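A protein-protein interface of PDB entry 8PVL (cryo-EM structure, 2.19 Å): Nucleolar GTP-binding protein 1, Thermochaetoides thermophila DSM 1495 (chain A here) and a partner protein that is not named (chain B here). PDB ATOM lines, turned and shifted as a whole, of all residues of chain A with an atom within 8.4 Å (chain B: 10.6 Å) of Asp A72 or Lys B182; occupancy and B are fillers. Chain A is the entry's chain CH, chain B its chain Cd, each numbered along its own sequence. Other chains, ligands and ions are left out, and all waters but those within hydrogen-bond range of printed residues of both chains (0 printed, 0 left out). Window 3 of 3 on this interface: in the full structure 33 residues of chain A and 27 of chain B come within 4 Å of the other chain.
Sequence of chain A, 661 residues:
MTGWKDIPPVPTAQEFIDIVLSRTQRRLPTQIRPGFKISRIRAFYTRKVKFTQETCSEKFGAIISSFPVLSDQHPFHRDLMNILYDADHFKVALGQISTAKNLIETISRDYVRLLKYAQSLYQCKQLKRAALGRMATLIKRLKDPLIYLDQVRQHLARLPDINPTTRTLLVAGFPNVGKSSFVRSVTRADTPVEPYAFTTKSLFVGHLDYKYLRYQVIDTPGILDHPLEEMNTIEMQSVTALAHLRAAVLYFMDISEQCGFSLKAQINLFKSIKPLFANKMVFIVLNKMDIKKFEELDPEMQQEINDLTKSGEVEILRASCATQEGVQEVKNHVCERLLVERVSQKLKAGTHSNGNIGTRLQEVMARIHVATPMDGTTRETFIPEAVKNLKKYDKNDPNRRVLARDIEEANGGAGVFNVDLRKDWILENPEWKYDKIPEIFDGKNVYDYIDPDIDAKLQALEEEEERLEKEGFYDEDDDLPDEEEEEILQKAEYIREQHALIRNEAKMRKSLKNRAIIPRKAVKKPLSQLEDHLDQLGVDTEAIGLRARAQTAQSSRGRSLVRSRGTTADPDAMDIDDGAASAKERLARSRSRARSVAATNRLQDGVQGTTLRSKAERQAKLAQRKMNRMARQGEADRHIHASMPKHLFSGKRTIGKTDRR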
ATOM      1  N   TRP A   4     -17.721 -20.888   2.931  1.00  0.00           N
ATOM      2  CA  TRP A   4     -18.203 -20.789   1.559  1.00  0.00           C
ATOM      3  C   TRP A   4     -19.721 -20.683   1.515  1.00  0.00           C
ATOM      4  O   TRP A   4     -20.355 -21.143   0.563  1.00  0.00           O
ATOM      5  CB  TRP A   4     -17.721 -21.979   0.731  1.00  0.00           C
ATOM      6  CG  TRP A   4     -16.260 -22.232   0.898  1.00  0.00           C
ATOM      7  CD1 TRP A   4     -15.677 -23.162   1.707  1.00  0.00           C
ATOM      8  CD2 TRP A   4     -15.193 -21.520   0.268  1.00  0.00           C
ATOM      9  NE1 TRP A   4     -14.311 -23.083   1.607  1.00  0.00           N
ATOM     10  CE2 TRP A   4     -13.988 -22.082   0.729  1.00  0.00           C
ATOM     11  CE3 TRP A   4     -15.139 -20.466  -0.648  1.00  0.00           C
ATOM     12  CZ2 TRP A   4     -12.744 -21.625   0.306  1.00  0.00           C
ATOM     13  CZ3 TRP A   4     -13.903 -20.015  -1.067  1.00  0.00           C
ATOM     14  CH2 TRP A   4     -12.722 -20.592  -0.587  1.00  0.00           C
ATOM     15  N   PHE A  67     -17.005 -19.833  -6.352  1.00  0.00           N
ATOM     16  CA  PHE A  67     -16.524 -21.147  -5.963  1.00  0.00           C
ATOM     17  C   PHE A  67     -15.043 -21.086  -5.591  1.00  0.00           C
ATOM     18  O   PHE A  67     -14.302 -20.247  -6.109  1.00  0.00           O
ATOM     19  CB  PHE A  67     -16.745 -22.152  -7.090  1.00  0.00           C
ATOM     20  CG  PHE A  67     -18.041 -22.903  -6.982  1.00  0.00           C
ATOM     21  CD1 PHE A  67     -19.221 -22.343  -7.440  1.00  0.00           C
ATOM     22  CD2 PHE A  67     -18.081 -24.162  -6.409  1.00  0.00           C
ATOM     23  CE1 PHE A  67     -20.416 -23.028  -7.337  1.00  0.00           C
ATOM     24  CE2 PHE A  67     -19.273 -24.852  -6.301  1.00  0.00           C
ATOM     25  CZ  PHE A  67     -20.441 -24.284  -6.765  1.00  0.00           C
ATOM     26  N   PRO A  68     -14.603 -21.937  -4.662  1.00  0.00           N
ATOM     27  CA  PRO A  68     -13.186 -21.949  -4.279  1.00  0.00           C
ATOM     28  C   PRO A  68     -12.276 -22.344  -5.432  1.00  0.00           C
ATOM     29  O   PRO A  68     -12.626 -23.171  -6.277  1.00  0.00           O
ATOM     30  CB  PRO A  68     -13.126 -22.989  -3.151  1.00  0.00           C
ATOM     31  CG  PRO A  68     -14.429 -23.711  -3.191  1.00  0.00           C
ATOM     32  CD  PRO A  68     -15.421 -22.762  -3.759  1.00  0.00           C
ATOM     33  N   VAL A  69     -11.099 -21.733  -5.458  1.00  0.00           N
ATOM     34  CA  VAL A  69     -10.040 -22.089  -6.392  1.00  0.00           C
ATOM     35  C   VAL A  69      -9.160 -23.109  -5.685  1.00  0.00           C
ATOM     36  O   VAL A  69      -8.527 -22.793  -4.674  1.00  0.00           O
ATOM     37  CB  VAL A  69      -9.234 -20.862  -6.837  1.00  0.00           C
ATOM     38  CG1 VAL A  69      -8.064 -21.285  -7.705  1.00  0.00           C
ATOM     39  CG2 VAL A  69     -10.127 -19.885  -7.581  1.00  0.00           C
ATOM     40  N   LEU A  70      -9.131 -24.334  -6.219  1.00  0.00           N
ATOM     41  CA  LEU A  70      -8.464 -25.445  -5.547  1.00  0.00           C
ATOM     42  C   LEU A  70      -6.960 -25.223  -5.440  1.00  0.00           C
ATOM     43  O   LEU A  70      -6.344 -25.581  -4.430  1.00  0.00           O
ATOM     44  CB  LEU A  70      -8.761 -26.749  -6.285  1.00  0.00           C
ATOM     45  CG  LEU A  70      -9.764 -27.719  -5.660  1.00  0.00           C
ATOM     46  CD1 LEU A  70     -11.005 -27.001  -5.183  1.00  0.00           C
ATOM     47  CD2 LEU A  70     -10.133 -28.785  -6.673  1.00  0.00           C
ATOM     48  N   SER A  71      -6.354 -24.627  -6.467  1.00  0.00           N
ATOM     49  CA  SER A  71      -4.917 -24.386  -6.458  1.00  0.00           C
ATOM     50  C   SER A  71      -4.504 -23.312  -5.458  1.00  0.00           C
ATOM     51  O   SER A  71      -3.322 -23.233  -5.112  1.00  0.00           O
ATOM     52  CB  SER A  71      -4.447 -23.996  -7.858  1.00  0.00           C
ATOM     53  OG  SER A  71      -4.744 -25.017  -8.792  1.00  0.00           O
ATOM     54  N   ASP A  72      -5.440 -22.492  -4.988  1.00  0.00           N
ATOM     55  CA  ASP A  72      -5.138 -21.408  -4.065  1.00  0.00           C
ATOM     56  C   ASP A  72      -5.430 -21.751  -2.611  1.00  0.00           C
ATOM     57  O   ASP A  72      -5.258 -20.889  -1.744  1.00  0.00           O
ATOM     58  CB  ASP A  72      -5.921 -20.152  -4.457  1.00  0.00           C
ATOM     59  CG  ASP A  72      -5.487 -19.590  -5.792  1.00  0.00           C
ATOM     60  OD1 ASP A  72      -4.455 -20.050  -6.323  1.00  0.00           O
ATOM     61  OD2 ASP A  72      -6.176 -18.688  -6.313  1.00  0.00           O
ATOM     62  N   GLN A  73      -5.867 -22.969  -2.318  1.00  0.00           N
ATOM     63  CA  GLN A  73      -6.202 -23.332  -0.950  1.00  0.00           C
ATOM     64  C   GLN A  73      -4.983 -23.865  -0.208  1.00  0.00           C
ATOM     65  O   GLN A  73      -3.961 -24.215  -0.802  1.00  0.00           O
ATOM     66  CB  GLN A  73      -7.316 -24.379  -0.915  1.00  0.00           C
ATOM     67  CG  GLN A  73      -8.564 -23.993  -1.674  1.00  0.00           C
ATOM     68  CD  GLN A  73      -9.238 -22.767  -1.097  1.00  0.00           C
ATOM     69  OE1 GLN A  73      -9.499 -22.695   0.103  1.00  0.00           O
ATOM     70  NE2 GLN A  73      -9.513 -21.788  -1.947  1.00  0.00           N
ATOM     71  N   HIS A  74      -5.109 -23.907   1.115  1.00  0.00           N
ATOM     72  CA  HIS A  74      -4.185 -24.667   1.937  1.00  0.00           C
ATOM     73  C   HIS A  74      -4.308 -26.144   1.564  1.00  0.00           C
ATOM     74  O   HIS A  74      -5.385 -26.591   1.159  1.00  0.00           O
ATOM     75  CB  HIS A  74      -4.506 -24.446   3.416  1.00  0.00           C
ATOM     76  CG  HIS A  74      -3.491 -25.012   4.358  1.00  0.00           C
ATOM     77  ND1 HIS A  74      -3.486 -26.336   4.739  1.00  0.00           N
ATOM     78  CD2 HIS A  74      -2.446 -24.435   4.995  1.00  0.00           C
ATOM     79  CE1 HIS A  74      -2.484 -26.550   5.571  1.00  0.00           C
ATOM     80  NE2 HIS A  74      -1.837 -25.412   5.743  1.00  0.00           N
ATOM     81  N   PRO A  75      -3.210 -26.910   1.641  1.00  0.00           N
ATOM     82  CA  PRO A  75      -3.267 -28.327   1.231  1.00  0.00           C
ATOM     83  C   PRO A  75      -4.299 -29.161   1.973  1.00  0.00           C
ATOM     84  O   PRO A  75      -4.836 -30.113   1.392  1.00  0.00           O
ATOM     85  CB  PRO A  75      -1.843 -28.819   1.513  1.00  0.00           C
ATOM     86  CG  PRO A  75      -1.002 -27.618   1.324  1.00  0.00           C
ATOM     87  CD  PRO A  75      -1.819 -26.436   1.766  1.00  0.00           C
ATOM     88  N   HIS A  77      -7.341 -28.022   2.922  1.00  0.00           N
ATOM     89  CA  HIS A  77      -8.623 -27.722   2.295  1.00  0.00           C
ATOM     90  C   HIS A  77      -8.696 -28.282   0.881  1.00  0.00           C
ATOM     91  O   HIS A  77      -9.747 -28.775   0.461  1.00  0.00           O
ATOM     92  CB  HIS A  77      -8.867 -26.215   2.288  1.00  0.00           C
ATOM     93  CG  HIS A  77      -9.161 -25.645   3.640  1.00  0.00           C
ATOM     94  ND1 HIS A  77     -10.197 -26.097   4.426  1.00  0.00           N
ATOM     95  CD2 HIS A  77      -8.553 -24.662   4.344  1.00  0.00           C
ATOM     96  CE1 HIS A  77     -10.216 -25.416   5.558  1.00  0.00           C
ATOM     97  NE2 HIS A  77      -9.229 -24.540   5.533  1.00  0.00           N
ATOM     98  N   ARG A  78      -7.585 -28.226   0.144  1.00  0.00           N
ATOM     99  CA  ARG A  78      -7.538 -28.781  -1.205  1.00  0.00           C
ATOM    100  C   ARG A  78      -7.760 -30.290  -1.190  1.00  0.00           C
ATOM    101  O   ARG A  78      -8.580 -30.821  -1.953  1.00  0.00           O
ATOM    102  CB  ARG A  78      -6.195 -28.434  -1.846  1.00  0.00           C
ATOM    103  CG  ARG A  78      -6.052 -28.811  -3.304  1.00  0.00           C
ATOM    104  CD  ARG A  78      -4.687 -28.383  -3.816  1.00  0.00           C
ATOM    105  NE  ARG A  78      -4.597 -28.409  -5.270  1.00  0.00           N
ATOM    106  CZ  ARG A  78      -3.603 -27.874  -5.965  1.00  0.00           C
ATOM    107  NH1 ARG A  78      -2.599 -27.253  -5.369  1.00  0.00           N
ATOM    108  NH2 ARG A  78      -3.619 -27.960  -7.292  1.00  0.00           N
ATOM    109  N   SER B 171       3.538 -30.318  -0.614  1.00  0.00           N
ATOM    110  CA  SER B 171       2.357 -29.486  -0.820  1.00  0.00           C
ATOM    111  C   SER B 171       2.403 -28.236   0.046  1.00  0.00           C
ATOM    112  O   SER B 171       2.086 -27.137  -0.424  1.00  0.00           O
ATOM    113  CB  SER B 171       1.091 -30.290  -0.528  1.00  0.00           C
ATOM    114  OG  SER B 171       0.882 -31.284  -1.513  1.00  0.00           O
ATOM    115  N   SER B 174       5.086 -25.897  -1.478  1.00  0.00           N
ATOM    116  CA  SER B 174       4.617 -25.221  -2.685  1.00  0.00           C
ATOM    117  C   SER B 174       3.561 -24.170  -2.361  1.00  0.00           C
ATOM    118  O   SER B 174       3.526 -23.106  -2.992  1.00  0.00           O
ATOM    119  CB  SER B 174       4.067 -26.243  -3.677  1.00  0.00           C
ATOM    120  OG  SER B 174       4.960 -27.331  -3.833  1.00  0.00           O
ATOM    121  N   TYR B 175       2.692 -24.452  -1.385  1.00  0.00           N
ATOM    122  CA  TYR B 175       1.693 -23.475  -0.964  1.00  0.00           C
ATOM    123  C   TYR B 175       2.347 -22.234  -0.368  1.00  0.00           C
ATOM    124  O   TYR B 175       1.944 -21.104  -0.671  1.00  0.00           O
ATOM    125  CB  TYR B 175       0.741 -24.129   0.038  1.00  0.00           C
ATOM    126  CG  TYR B 175      -0.192 -23.187   0.760  1.00  0.00           C
ATOM    127  CD1 TYR B 175      -1.262 -22.596   0.101  1.00  0.00           C
ATOM    128  CD2 TYR B 175      -0.020 -22.911   2.109  1.00  0.00           C
ATOM    129  CE1 TYR B 175      -2.124 -21.745   0.763  1.00  0.00           C
ATOM    130  CE2 TYR B 175      -0.878 -22.062   2.780  1.00  0.00           C
ATOM    131  CZ  TYR B 175      -1.928 -21.483   2.102  1.00  0.00           C
ATOM    132  OH  TYR B 175      -2.784 -20.637   2.764  1.00  0.00           O
ATOM    133  N   HIS B 176       3.376 -22.426   0.463  1.00  0.00           N
ATOM    134  CA  HIS B 176       4.087 -21.284   1.029  1.00  0.00           C
ATOM    135  C   HIS B 176       4.839 -20.503  -0.043  1.00  0.00           C
ATOM    136  O   HIS B 176       4.896 -19.269   0.010  1.00  0.00           O
ATOM    137  CB  HIS B 176       5.039 -21.747   2.129  1.00  0.00           C
ATOM    138  CG  HIS B 176       4.346 -22.146   3.393  1.00  0.00           C
ATOM    139  ND1 HIS B 176       3.239 -21.481   3.874  1.00  0.00           N
ATOM    140  CD2 HIS B 176       4.604 -23.137   4.278  1.00  0.00           C
ATOM    141  CE1 HIS B 176       2.844 -22.048   5.000  1.00  0.00           C
ATOM    142  NE2 HIS B 176       3.655 -23.054   5.267  1.00  0.00           N
ATOM    143  N   ALA B 177       5.416 -21.203  -1.027  1.00  0.00           N
ATOM    144  CA  ALA B 177       6.103 -20.518  -2.121  1.00  0.00           C
ATOM    145  C   ALA B 177       5.132 -19.693  -2.960  1.00  0.00           C
ATOM    146  O   ALA B 177       5.450 -18.565  -3.361  1.00  0.00           O
ATOM    147  CB  ALA B 177       6.836 -21.532  -2.996  1.00  0.00           C
ATOM    148  N   ARG B 178       3.945 -20.240  -3.234  1.00  0.00           N
ATOM    149  CA  ARG B 178       2.934 -19.498  -3.983  1.00  0.00           C
ATOM    150  C   ARG B 178       2.440 -18.285  -3.204  1.00  0.00           C
ATOM    151  O   ARG B 178       2.241 -17.209  -3.785  1.00  0.00           O
ATOM    152  CB  ARG B 178       1.766 -20.415  -4.340  1.00  0.00           C
ATOM    153  CG  ARG B 178       1.961 -21.191  -5.630  1.00  0.00           C
ATOM    154  CD  ARG B 178       0.625 -21.613  -6.214  1.00  0.00           C
ATOM    155  NE  ARG B 178      -0.343 -20.524  -6.186  1.00  0.00           N
ATOM    156  CZ  ARG B 178      -1.379 -20.421  -7.006  1.00  0.00           C
ATOM    157  NH1 ARG B 178      -1.620 -21.332  -7.934  1.00  0.00           N
ATOM    158  NH2 ARG B 178      -2.196 -19.378  -6.890  1.00  0.00           N
ATOM    159  N   LEU B 179       2.238 -18.435  -1.891  1.00  0.00           N
ATOM    160  CA  LEU B 179       1.842 -17.293  -1.069  1.00  0.00           C
ATOM    161  C   LEU B 179       2.920 -16.215  -1.052  1.00  0.00           C
ATOM    162  O   LEU B 179       2.610 -15.020  -1.126  1.00  0.00           O
ATOM    163  CB  LEU B 179       1.527 -17.741   0.356  1.00  0.00           C
ATOM    164  CG  LEU B 179       0.121 -18.269   0.624  1.00  0.00           C
ATOM    165  CD1 LEU B 179      -0.070 -18.487   2.110  1.00  0.00           C
ATOM    166  CD2 LEU B 179      -0.919 -17.311   0.079  1.00  0.00           C
ATOM    167  N   GLU B 180       4.192 -16.622  -0.961  1.00  0.00           N
ATOM    168  CA  GLU B 180       5.288 -15.657  -0.953  1.00  0.00           C
ATOM    169  C   GLU B 180       5.407 -14.929  -2.285  1.00  0.00           C
ATOM    170  O   GLU B 180       5.641 -13.716  -2.309  1.00  0.00           O
ATOM    171  CB  GLU B 180       6.610 -16.350  -0.602  1.00  0.00           C
ATOM    172  CG  GLU B 180       7.580 -15.582   0.346  1.00  0.00           C
ATOM    173  CD  GLU B 180       6.935 -14.910   1.575  1.00  0.00           C
ATOM    174  OE1 GLU B 180       7.568 -13.988   2.134  1.00  0.00           O
ATOM    175  OE2 GLU B 180       5.867 -15.350   2.061  1.00  0.00           O
ATOM    176  N   GLU B 181       5.233 -15.640  -3.404  1.00  0.00           N
ATOM    177  CA  GLU B 181       5.312 -14.965  -4.697  1.00  0.00           C
ATOM    178  C   GLU B 181       4.100 -14.071  -4.943  1.00  0.00           C
ATOM    179  O   GLU B 181       4.226 -13.032  -5.602  1.00  0.00           O
ATOM    180  CB  GLU B 181       5.501 -15.984  -5.830  1.00  0.00           C
ATOM    181  CG  GLU B 181       4.257 -16.738  -6.293  1.00  0.00           C
ATOM    182  CD  GLU B 181       3.593 -16.113  -7.510  1.00  0.00           C
ATOM    183  OE1 GLU B 181       4.066 -15.055  -7.973  1.00  0.00           O
ATOM    184  OE2 GLU B 181       2.592 -16.679  -8.002  1.00  0.00           O
ATOM    185  N   LYS B 182       2.930 -14.434  -4.401  1.00  0.00           N
ATOM    186  CA  LYS B 182       1.767 -13.559  -4.508  1.00  0.00           C
ATOM    187  C   LYS B 182       1.939 -12.305  -3.659  1.00  0.00           C
ATOM    188  O   LYS B 182       1.527 -11.213  -4.067  1.00  0.00           O
ATOM    189  CB  LYS B 182       0.502 -14.312  -4.100  1.00  0.00           C
ATOM    190  CG  LYS B 182      -0.239 -14.957  -5.258  1.00  0.00           C
ATOM    191  CD  LYS B 182      -1.741 -14.935  -5.028  1.00  0.00           C
ATOM    192  CE  LYS B 182      -2.302 -16.343  -4.904  1.00  0.00           C
ATOM    193  NZ  LYS B 182      -3.655 -16.351  -4.282  1.00  0.00           N
ATOM    194  N   LYS B 183       2.529 -12.448  -2.470  1.00  0.00           N
ATOM    195  CA  LYS B 183       2.803 -11.288  -1.626  1.00  0.00           C
ATOM    196  C   LYS B 183       3.855 -10.383  -2.255  1.00  0.00           C
ATOM    197  O   LYS B 183       3.740  -9.153  -2.196  1.00  0.00           O
ATOM    198  CB  LYS B 183       3.244 -11.753  -0.237  1.00  0.00           C
ATOM    199  CG  LYS B 183       3.727 -10.649   0.687  1.00  0.00           C
ATOM    200  CD  LYS B 183       4.258 -11.224   1.990  1.00  0.00           C
ATOM    201  CE  LYS B 183       4.848 -10.140   2.876  1.00  0.00           C
ATOM    202  NZ  LYS B 183       5.416 -10.702   4.132  1.00  0.00           N
ATOM    203  N   LEU B 184       4.883 -10.975  -2.870  1.00  0.00           N
ATOM    204  CA  LEU B 184       5.924 -10.185  -3.519  1.00  0.00           C
ATOM    205  C   LEU B 184       5.394  -9.479  -4.762  1.00  0.00           C
ATOM    206  O   LEU B 184       5.802  -8.351  -5.063  1.00  0.00           O
ATOM    207  CB  LEU B 184       7.112 -11.080  -3.870  1.00  0.00           C
ATOM    208  CG  LEU B 184       8.343 -10.414  -4.485  1.00  0.00           C
ATOM    209  CD1 LEU B 184       8.889  -9.339  -3.559  1.00  0.00           C
ATOM    210  CD2 LEU B 184       9.409 -11.450  -4.801  1.00  0.00           C
ATOM    211  N   LEU B 185       4.485 -10.120  -5.492  1.00  0.00           N
ATOM    212  CA  LEU B 185       3.887  -9.504  -6.672  1.00  0.00           C
ATOM    213  C   LEU B 185       2.932  -8.378  -6.286  1.00  0.00           C
ATOM    214  O   LEU B 185       2.459  -8.311  -5.151  1.00  0.00           O
ATOM    215  CB  LEU B 185       3.149 -10.552  -7.507  1.00  0.00           C
ATOM    216  CG  LEU B 185       2.413 -10.030  -8.743  1.00  0.00           C
ATOM    217  CD1 LEU B 185       3.384  -9.365  -9.706  1.00  0.00           C
ATOM    218  CD2 LEU B 185       1.652 -11.153  -9.430  1.00  0.00           C
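The side-chain amino group (NZ) of Lys B182 is in salt-bridge range of the side-chain carboxylate (OD2) of Asp A72, 3.99 Å away.
NH2 of Arg B178 lies within salt-bridge range of OD1 of Asp A72.
OG of Ser A71 lies within hydrogen-bond range of NH2 of Arg A78 (3.5 Å).
The backbone carbonyl oxygen (O) of Val A69 lies within hydrogen-bond range of the side-chain amide nitrogen (NE2) of Gln A73.
Among the printed residues, merely in contact across the chains: Ser A71 with Arg B178, Gln A73 with Tyr B175, His A74 with Tyr B175, Pro A75 with Ser B171 and Pro A75 with Tyr B175.
Of the printed residues of chain A, Lys B182 touches Asp A72.
No residue of chain B comes within 4 Å of Val A69.
Of chain B, only Arg B178 (3.8 Å) comes within 4 Å of Ser A71.
Of chain B, only Tyr B175 comes within 4 Å of Gln A73.
No residue of chain A comes within 4 Å of Glu B181.
Printed residues of chain B within 4 Å of His A74: Tyr B175.
Of the printed residues of chain A, Tyr B175 touches Gln A73, His A74 and Pro A75.
Printed residues of chain B within 4 Å of Pro A75: Ser B171 and Tyr B175.
Printed residues of chain A within 4 Å of Arg B178: Ser A71 (3.8 Å) and Asp A72 (2.4 Å).
Lys B183 touches none of the printed residues of chain A.
The nearest printed residue of chain B that does not touch Asp A72 is Tyr B175 (4.1 Å).
Hydrophobic or aromatic side chains of chain A within 4 Å of the printed part of chain B: His A74 and Pro A75.
Of the 13 printed residues of chain B, 4 touch a printed residue of chain A.
Printed residues of chain B that touch a printed residue of chain A: Ser B171, Tyr B175, Arg B178 and Lys B182.
Among the printed residues, 7 pairs touch across the chains.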
